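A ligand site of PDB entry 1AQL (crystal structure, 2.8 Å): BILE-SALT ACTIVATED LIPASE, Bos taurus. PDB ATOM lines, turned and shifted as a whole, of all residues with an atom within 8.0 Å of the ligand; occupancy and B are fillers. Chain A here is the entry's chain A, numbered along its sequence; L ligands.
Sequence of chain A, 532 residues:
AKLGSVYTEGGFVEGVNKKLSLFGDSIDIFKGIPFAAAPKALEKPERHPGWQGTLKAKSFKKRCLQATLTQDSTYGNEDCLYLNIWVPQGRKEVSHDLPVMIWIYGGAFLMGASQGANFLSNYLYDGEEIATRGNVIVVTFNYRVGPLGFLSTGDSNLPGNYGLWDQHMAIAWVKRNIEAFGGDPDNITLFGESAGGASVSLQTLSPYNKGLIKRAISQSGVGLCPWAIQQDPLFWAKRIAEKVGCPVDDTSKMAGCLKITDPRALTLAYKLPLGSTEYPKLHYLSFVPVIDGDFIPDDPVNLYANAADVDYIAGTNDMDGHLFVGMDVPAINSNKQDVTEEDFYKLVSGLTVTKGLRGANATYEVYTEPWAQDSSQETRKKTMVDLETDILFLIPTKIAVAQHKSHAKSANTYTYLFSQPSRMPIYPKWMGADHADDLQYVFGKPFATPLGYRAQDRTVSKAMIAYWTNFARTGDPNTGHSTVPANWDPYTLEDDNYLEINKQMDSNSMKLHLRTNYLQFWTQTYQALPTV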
ATOM      1  N   GLN A 115     -21.452  14.478   9.276  1.00  0.00           N
ATOM      2  CA  GLN A 115     -22.402  13.373   9.356  1.00  0.00           C
ATOM      3  C   GLN A 115     -21.697  12.018   9.460  1.00  0.00           C
ATOM      4  O   GLN A 115     -22.226  11.084  10.047  1.00  0.00           O
ATOM      5  CB  GLN A 115     -23.307  13.381   8.115  1.00  0.00           C
ATOM      6  CG  GLN A 115     -22.563  13.436   6.792  1.00  0.00           C
ATOM      7  CD  GLN A 115     -22.942  14.664   5.958  1.00  0.00           C
ATOM      8  OE1 GLN A 115     -23.215  14.548   4.764  1.00  0.00           O
ATOM      9  NE2 GLN A 115     -22.961  15.841   6.572  1.00  0.00           N
ATOM     10  N   GLY A 116     -20.497  11.951   8.915  1.00  0.00           N
ATOM     11  CA  GLY A 116     -19.748  10.703   8.923  1.00  0.00           C
ATOM     12  C   GLY A 116     -20.337   9.778   7.887  1.00  0.00           C
ATOM     13  O   GLY A 116     -21.539   9.832   7.645  1.00  0.00           O
ATOM     14  N   ALA A 117     -19.488   8.972   7.244  1.00  0.00           N
ATOM     15  CA  ALA A 117     -19.915   8.019   6.205  1.00  0.00           C
ATOM     16  C   ALA A 117     -21.158   7.293   6.631  1.00  0.00           C
ATOM     17  O   ALA A 117     -21.352   7.033   7.814  1.00  0.00           O
ATOM     18  CB  ALA A 117     -18.821   7.011   5.923  1.00  0.00           C
ATOM     19  N   ASN A 118     -21.973   6.924   5.660  1.00  0.00           N
ATOM     20  CA  ASN A 118     -23.198   6.238   5.987  1.00  0.00           C
ATOM     21  C   ASN A 118     -23.607   5.188   4.963  1.00  0.00           C
ATOM     22  O   ASN A 118     -22.998   5.060   3.886  1.00  0.00           O
ATOM     23  CB  ASN A 118     -24.359   7.233   6.227  1.00  0.00           C
ATOM     24  CG  ASN A 118     -24.821   7.934   4.946  1.00  0.00           C
ATOM     25  OD1 ASN A 118     -25.676   7.433   4.223  1.00  0.00           O
ATOM     26  ND2 ASN A 118     -24.299   9.126   4.709  1.00  0.00           N
ATOM     27  N   PHE A 119     -24.559   4.369   5.394  1.00  0.00           N
ATOM     28  CA  PHE A 119     -25.135   3.324   4.567  1.00  0.00           C
ATOM     29  C   PHE A 119     -26.596   3.297   4.968  1.00  0.00           C
ATOM     30  O   PHE A 119     -26.923   2.885   6.077  1.00  0.00           O
ATOM     31  CB  PHE A 119     -24.511   1.970   4.857  1.00  0.00           C
ATOM     32  CG  PHE A 119     -25.178   0.835   4.122  1.00  0.00           C
ATOM     33  CD1 PHE A 119     -24.810   0.537   2.821  1.00  0.00           C
ATOM     34  CD2 PHE A 119     -26.193   0.100   4.740  1.00  0.00           C
ATOM     35  CE1 PHE A 119     -25.443  -0.490   2.133  1.00  0.00           C
ATOM     36  CE2 PHE A 119     -26.829  -0.934   4.058  1.00  0.00           C
ATOM     37  CZ  PHE A 119     -26.448  -1.226   2.753  1.00  0.00           C
ATOM     38  N   LEU A 120     -27.442   3.838   4.096  1.00  0.00           N
ATOM     39  CA  LEU A 120     -28.872   3.863   4.357  1.00  0.00           C
ATOM     40  C   LEU A 120     -29.153   4.510   5.701  1.00  0.00           C
ATOM     41  O   LEU A 120     -29.575   3.832   6.641  1.00  0.00           O
ATOM     42  CB  LEU A 120     -29.438   2.445   4.325  1.00  0.00           C
ATOM     43  CG  LEU A 120     -29.535   1.801   2.940  1.00  0.00           C
ATOM     44  CD1 LEU A 120     -30.494   2.626   2.108  1.00  0.00           C
ATOM     45  CD2 LEU A 120     -28.164   1.735   2.278  1.00  0.00           C
ATOM     46  N   SER A 121     -28.843   5.787   5.808  1.00  0.00           N
ATOM     47  CA  SER A 121     -29.067   6.539   7.044  1.00  0.00           C
ATOM     48  C   SER A 121     -28.240   6.093   8.248  1.00  0.00           C
ATOM     49  O   SER A 121     -28.454   6.583   9.365  1.00  0.00           O
ATOM     50  CB  SER A 121     -30.559   6.577   7.408  1.00  0.00           C
ATOM     51  OG  SER A 121     -31.320   7.223   6.398  1.00  0.00           O
ATOM     52  N   ASN A 122     -27.297   5.181   8.039  1.00  0.00           N
ATOM     53  CA  ASN A 122     -26.463   4.720   9.144  1.00  0.00           C
ATOM     54  C   ASN A 122     -25.216   5.592   9.198  1.00  0.00           C
ATOM     55  O   ASN A 122     -24.160   5.223   8.720  1.00  0.00           O
ATOM     56  CB  ASN A 122     -26.082   3.243   8.976  1.00  0.00           C
ATOM     57  CG  ASN A 122     -25.533   2.646  10.250  1.00  0.00           C
ATOM     58  OD1 ASN A 122     -25.855   3.109  11.353  1.00  0.00           O
ATOM     59  ND2 ASN A 122     -24.708   1.614  10.123  1.00  0.00           N
ATOM     60  N   TYR A 123     -25.395   6.790   9.749  1.00  0.00           N
ATOM     61  CA  TYR A 123     -24.325   7.801   9.892  1.00  0.00           C
ATOM     62  C   TYR A 123     -23.247   7.475  10.926  1.00  0.00           C
ATOM     63  O   TYR A 123     -23.489   7.558  12.145  1.00  0.00           O
ATOM     64  CB  TYR A 123     -24.948   9.170  10.201  1.00  0.00           C
ATOM     65  CG  TYR A 123     -25.818   9.697   9.087  1.00  0.00           C
ATOM     66  CD1 TYR A 123     -25.257  10.152   7.902  1.00  0.00           C
ATOM     67  CD2 TYR A 123     -27.205   9.750   9.219  1.00  0.00           C
ATOM     68  CE1 TYR A 123     -26.039  10.630   6.865  1.00  0.00           C
ATOM     69  CE2 TYR A 123     -28.009  10.226   8.185  1.00  0.00           C
ATOM     70  CZ  TYR A 123     -27.409  10.673   7.008  1.00  0.00           C
ATOM     71  OH  TYR A 123     -28.182  11.156   5.980  1.00  0.00           O
ATOM     72  N   LEU A 124     -22.038   7.225  10.440  1.00  0.00           N
ATOM     73  CA  LEU A 124     -20.891   6.873  11.273  1.00  0.00           C
ATOM     74  C   LEU A 124     -20.680   7.740  12.500  1.00  0.00           C
ATOM     75  O   LEU A 124     -20.021   7.333  13.452  1.00  0.00           O
ATOM     76  CB  LEU A 124     -19.616   6.866  10.437  1.00  0.00           C
ATOM     77  CG  LEU A 124     -18.398   6.261  11.113  1.00  0.00           C
ATOM     78  CD1 LEU A 124     -18.721   4.822  11.442  1.00  0.00           C
ATOM     79  CD2 LEU A 124     -17.160   6.342  10.245  1.00  0.00           C
ATOM     80  N   TYR A 125     -21.192   8.966  12.484  1.00  0.00           N
ATOM     81  CA  TYR A 125     -21.015   9.841  13.632  1.00  0.00           C
ATOM     82  C   TYR A 125     -22.345  10.290  14.203  1.00  0.00           C
ATOM     83  O   TYR A 125     -22.454  11.400  14.728  1.00  0.00           O
ATOM     84  CB  TYR A 125     -20.155  11.055  13.255  1.00  0.00           C
ATOM     85  CG  TYR A 125     -18.776  10.747  12.697  1.00  0.00           C
ATOM     86  CD1 TYR A 125     -18.234   9.471  12.765  1.00  0.00           C
ATOM     87  CD2 TYR A 125     -18.030  11.735  12.080  1.00  0.00           C
ATOM     88  CE1 TYR A 125     -16.990   9.185  12.229  1.00  0.00           C
ATOM     89  CE2 TYR A 125     -16.786  11.456  11.551  1.00  0.00           C
ATOM     90  CZ  TYR A 125     -16.276  10.180  11.620  1.00  0.00           C
ATOM     91  OH  TYR A 125     -15.048   9.890  11.059  1.00  0.00           O
ATOM     92  N   ASP A 126     -23.359   9.433  14.102  1.00  0.00           N
ATOM     93  CA  ASP A 126     -24.685   9.766  14.634  1.00  0.00           C
ATOM     94  C   ASP A 126     -24.521   9.800  16.155  1.00  0.00           C
ATOM     95  O   ASP A 126     -24.263   8.775  16.784  1.00  0.00           O
ATOM     96  CB  ASP A 126     -25.729   8.716  14.231  1.00  0.00           C
ATOM     97  CG  ASP A 126     -27.181   9.174  14.451  1.00  0.00           C
ATOM     98  OD1 ASP A 126     -27.452  10.004  15.350  1.00  0.00           O
ATOM     99  OD2 ASP A 126     -28.072   8.688  13.714  1.00  0.00           O
ATOM    100  N   GLN A 440     -16.329   3.149  15.667  1.00  0.00           N
ATOM    101  CA  GLN A 440     -17.584   2.428  15.859  1.00  0.00           C
ATOM    102  C   GLN A 440     -17.917   2.152  17.331  1.00  0.00           C
ATOM    103  O   GLN A 440     -19.067   2.267  17.741  1.00  0.00           O
ATOM    104  CB  GLN A 440     -17.545   1.111  15.103  1.00  0.00           C
ATOM    105  CG  GLN A 440     -16.316   0.312  15.433  1.00  0.00           C
ATOM    106  CD  GLN A 440     -16.135  -0.831  14.483  1.00  0.00           C
ATOM    107  OE1 GLN A 440     -17.067  -1.229  13.785  1.00  0.00           O
ATOM    108  NE2 GLN A 440     -14.930  -1.382  14.446  1.00  0.00           N
ATOM    109  N   LYS A 445     -22.026   2.034  17.696  1.00  0.00           N
ATOM    110  CA  LYS A 445     -22.361   1.266  16.512  1.00  0.00           C
ATOM    111  C   LYS A 445     -22.810  -0.174  16.843  1.00  0.00           C
ATOM    112  O   LYS A 445     -23.727  -0.677  16.209  1.00  0.00           O
ATOM    113  CB  LYS A 445     -21.194   1.291  15.530  1.00  0.00           C
ATOM    114  CG  LYS A 445     -21.585   1.045  14.071  1.00  0.00           C
ATOM    115  CD  LYS A 445     -22.692   1.992  13.616  1.00  0.00           C
ATOM    116  CE  LYS A 445     -22.328   3.452  13.852  1.00  0.00           C
ATOM    117  NZ  LYS A 445     -23.543   4.309  13.861  1.00  0.00           N
ATOM    118  N   PRO A 446     -22.185  -0.835  17.839  1.00  0.00           N
ATOM    119  CA  PRO A 446     -22.581  -2.214  18.180  1.00  0.00           C
ATOM    120  C   PRO A 446     -24.026  -2.333  18.703  1.00  0.00           C
ATOM    121  O   PRO A 446     -24.657  -3.389  18.616  1.00  0.00           O
ATOM    122  CB  PRO A 446     -21.565  -2.591  19.254  1.00  0.00           C
ATOM    123  CG  PRO A 446     -20.365  -1.863  18.841  1.00  0.00           C
ATOM    124  CD  PRO A 446     -20.935  -0.499  18.555  1.00  0.00           C
ATOM    125  N   ALA A 448     -26.444   0.271  17.915  1.00  0.00           N
ATOM    126  CA  ALA A 448     -27.295   0.865  16.875  1.00  0.00           C
ATOM    127  C   ALA A 448     -27.505  -0.141  15.746  1.00  0.00           C
ATOM    128  O   ALA A 448     -28.575  -0.177  15.137  1.00  0.00           O
ATOM    129  CB  ALA A 448     -26.655   2.121  16.343  1.00  0.00           C
ATOM    130  N   THR A 449     -26.493  -0.951  15.461  1.00  0.00           N
ATOM    131  CA  THR A 449     -26.580  -1.970  14.430  1.00  0.00           C
ATOM    132  C   THR A 449     -26.049  -3.307  14.975  1.00  0.00           C
ATOM    133  O   THR A 449     -25.054  -3.843  14.468  1.00  0.00           O
ATOM    134  CB  THR A 449     -25.805  -1.552  13.138  1.00  0.00           C
ATOM    135  OG1 THR A 449     -25.676  -2.678  12.257  1.00  0.00           O
ATOM    136  CG2 THR A 449     -24.418  -1.047  13.479  1.00  0.00           C
ATOM    137  N   PRO A 450     -26.734  -3.886  15.973  1.00  0.00           N
ATOM    138  CA  PRO A 450     -26.378  -5.164  16.617  1.00  0.00           C
ATOM    139  C   PRO A 450     -25.946  -6.297  15.682  1.00  0.00           C
ATOM    140  O   PRO A 450     -24.857  -6.846  15.845  1.00  0.00           O
ATOM    141  CB  PRO A 450     -27.646  -5.520  17.393  1.00  0.00           C
ATOM    142  CG  PRO A 450     -28.124  -4.176  17.828  1.00  0.00           C
ATOM    143  CD  PRO A 450     -27.998  -3.371  16.548  1.00  0.00           C
ATOM    144  N   LEU A 451     -26.792  -6.689  14.734  1.00  0.00           N
ATOM    145  CA  LEU A 451     -26.421  -7.758  13.806  1.00  0.00           C
ATOM    146  C   LEU A 451     -25.100  -7.343  13.139  1.00  0.00           C
ATOM    147  O   LEU A 451     -24.993  -6.238  12.597  1.00  0.00           O
ATOM    148  CB  LEU A 451     -27.515  -7.987  12.765  1.00  0.00           C
ATOM    149  CG  LEU A 451     -27.355  -9.183  11.813  1.00  0.00           C
ATOM    150  CD1 LEU A 451     -27.591 -10.500  12.545  1.00  0.00           C
ATOM    151  CD2 LEU A 451     -28.323  -9.054  10.648  1.00  0.00           C
ATOM    152  N   GLY A 452     -24.101  -8.212  13.201  1.00  0.00           N
ATOM    153  CA  GLY A 452     -22.802  -7.880  12.648  1.00  0.00           C
ATOM    154  C   GLY A 452     -21.878  -7.507  13.801  1.00  0.00           C
ATOM    155  O   GLY A 452     -20.736  -7.102  13.618  1.00  0.00           O
ATOM    156  N   TYR A 453     -22.415  -7.628  15.016  1.00  0.00           N
ATOM    157  CA  TYR A 453     -21.710  -7.354  16.257  1.00  0.00           C
ATOM    158  C   TYR A 453     -22.033  -8.445  17.289  1.00  0.00           C
ATOM    159  O   TYR A 453     -23.131  -9.024  17.278  1.00  0.00           O
ATOM    160  CB  TYR A 453     -22.112  -5.977  16.814  1.00  0.00           C
ATOM    161  CG  TYR A 453     -21.529  -4.800  16.078  1.00  0.00           C
ATOM    162  CD1 TYR A 453     -20.155  -4.542  16.128  1.00  0.00           C
ATOM    163  CD2 TYR A 453     -22.334  -3.923  15.363  1.00  0.00           C
ATOM    164  CE1 TYR A 453     -19.608  -3.445  15.475  1.00  0.00           C
ATOM    165  CE2 TYR A 453     -21.796  -2.817  14.714  1.00  0.00           C
ATOM    166  CZ  TYR A 453     -20.431  -2.586  14.778  1.00  0.00           C
ATOM    167  OH  TYR A 453     -19.896  -1.486  14.136  1.00  0.00           O
HETATM  168  C1  LIG L   1     -21.636   1.261   7.220  1.00  0.00           C
HETATM  169  C2  LIG L   1     -21.084   2.584   7.665  1.00  0.00           C
HETATM  170  C3  LIG L   1     -21.613   2.865   9.013  1.00  0.00           C
HETATM  171  O1  LIG L   1     -21.744   4.228   9.409  1.00  0.00           O
HETATM  172  C4  LIG L   1     -20.963   1.795   9.912  1.00  0.00           C
HETATM  173  C5  LIG L   1     -21.572   0.433   9.551  1.00  0.00           C
HETATM  174  C6  LIG L   1     -21.240  -0.705  10.452  1.00  0.00           C
HETATM  175  C7  LIG L   1     -22.183  -1.866  10.247  1.00  0.00           C
HETATM  176  O2  LIG L   1     -23.517  -1.668  10.673  1.00  0.00           O
HETATM  177  C8  LIG L   1     -22.204  -2.388   8.779  1.00  0.00           C
HETATM  178  C9  LIG L   1     -22.085  -1.143   7.736  1.00  0.00           C
HETATM  179  C10 LIG L   1     -21.259   0.099   8.132  1.00  0.00           C
HETATM  180  C11 LIG L   1     -22.662  -1.032   6.386  1.00  0.00           C
HETATM  181  C12 LIG L   1     -23.821  -2.077   6.479  1.00  0.00           C
HETATM  182  O3  LIG L   1     -25.175  -1.708   6.931  1.00  0.00           O
HETATM  183  C13 LIG L   1     -23.453  -3.557   6.857  1.00  0.00           C
HETATM  184  C14 LIG L   1     -23.269  -3.499   8.410  1.00  0.00           C
HETATM  185  C15 LIG L   1     -23.560  -4.819   9.203  1.00  0.00           C
HETATM  186  C16 LIG L   1     -24.458  -5.517   8.182  1.00  0.00           C
HETATM  187  C17 LIG L   1     -24.609  -4.653   6.887  1.00  0.00           C
HETATM  188  C18 LIG L   1     -22.061  -4.107   6.288  1.00  0.00           C
HETATM  189  C19 LIG L   1     -19.813  -0.212   7.847  1.00  0.00           C
HETATM  190  O4  LIG L   1     -23.722  -9.550  -0.256  1.00  0.00           O
HETATM  191  C20 LIG L   1     -25.207  -5.486   5.644  1.00  0.00           C
HETATM  192  C21 LIG L   1     -26.686  -5.360   5.646  1.00  0.00           C
HETATM  193  C22 LIG L   1     -24.653  -5.099   4.228  1.00  0.00           C
HETATM  194  C23 LIG L   1     -24.045  -6.212   3.271  1.00  0.00           C
HETATM  195  C24 LIG L   1     -25.098  -7.266   2.858  1.00  0.00           C
HETATM  196  N1  LIG L   1     -24.697  -8.219   1.911  1.00  0.00           N
HETATM  197  O5  LIG L   1     -25.894  -7.733   3.758  1.00  0.00           O
HETATM  198  C25 LIG L   1     -24.768  -9.683   2.206  1.00  0.00           C
HETATM  199  C26 LIG L   1     -25.446 -10.697   1.205  1.00  0.00           C
HETATM  200  S1  LIG L   1     -25.055 -10.055  -0.412  1.00  0.00           S
HETATM  201  O6  LIG L   1     -25.135 -10.936  -1.627  1.00  0.00           O
HETATM  202  O7  LIG L   1     -25.955  -8.916  -0.607  1.00  0.00           O
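CD2 of Phe 119 touches O3 of the ligand, at 3.0 Å. C of Tyr 123 touches O1 of the ligand (3.9 Å). O of Leu 451 touches C15 of the ligand, at 3.9 Å. Tyr 453 touches the ligand (OH to C6, 3.999 Å). Within 4 Å of the ligand: Ala 117, Phe 119, Asn 122, Tyr 123, Leu 124, Thr 449, Leu 451 and Tyr 453. The nearest printed residue that does not touch the ligand is Lys 445 (4.03 Å).
An oxygen (O1) of the ligand sits at hydrogen-bond distance from the backbone carbonyl oxygen (O) of Asn 122, at 2.7 Å. OG1 of Thr 449 lies within hydrogen-bond range of O2 of the ligand, at 2.9 Å. The backbone NH (N) of Leu 124 sits at hydrogen-bond distance from an oxygen (O1) of the ligand, 3.2 Å away. The backbone carbonyl oxygen (O) of Ala 117 is in hydrogen-bond range of an oxygen (O1) of the ligand, at 3.3 Å.
The backbone carbonyl oxygen of Ala 117 lies within hydrogen-bond range of the backbone NH of Leu 124 (2.7 Å). The side-chain hydroxyl (OH) of Tyr 453 sits at hydrogen-bond distance from the side-chain amide oxygen (OE1) of Gln 440, 2.9 Å away.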
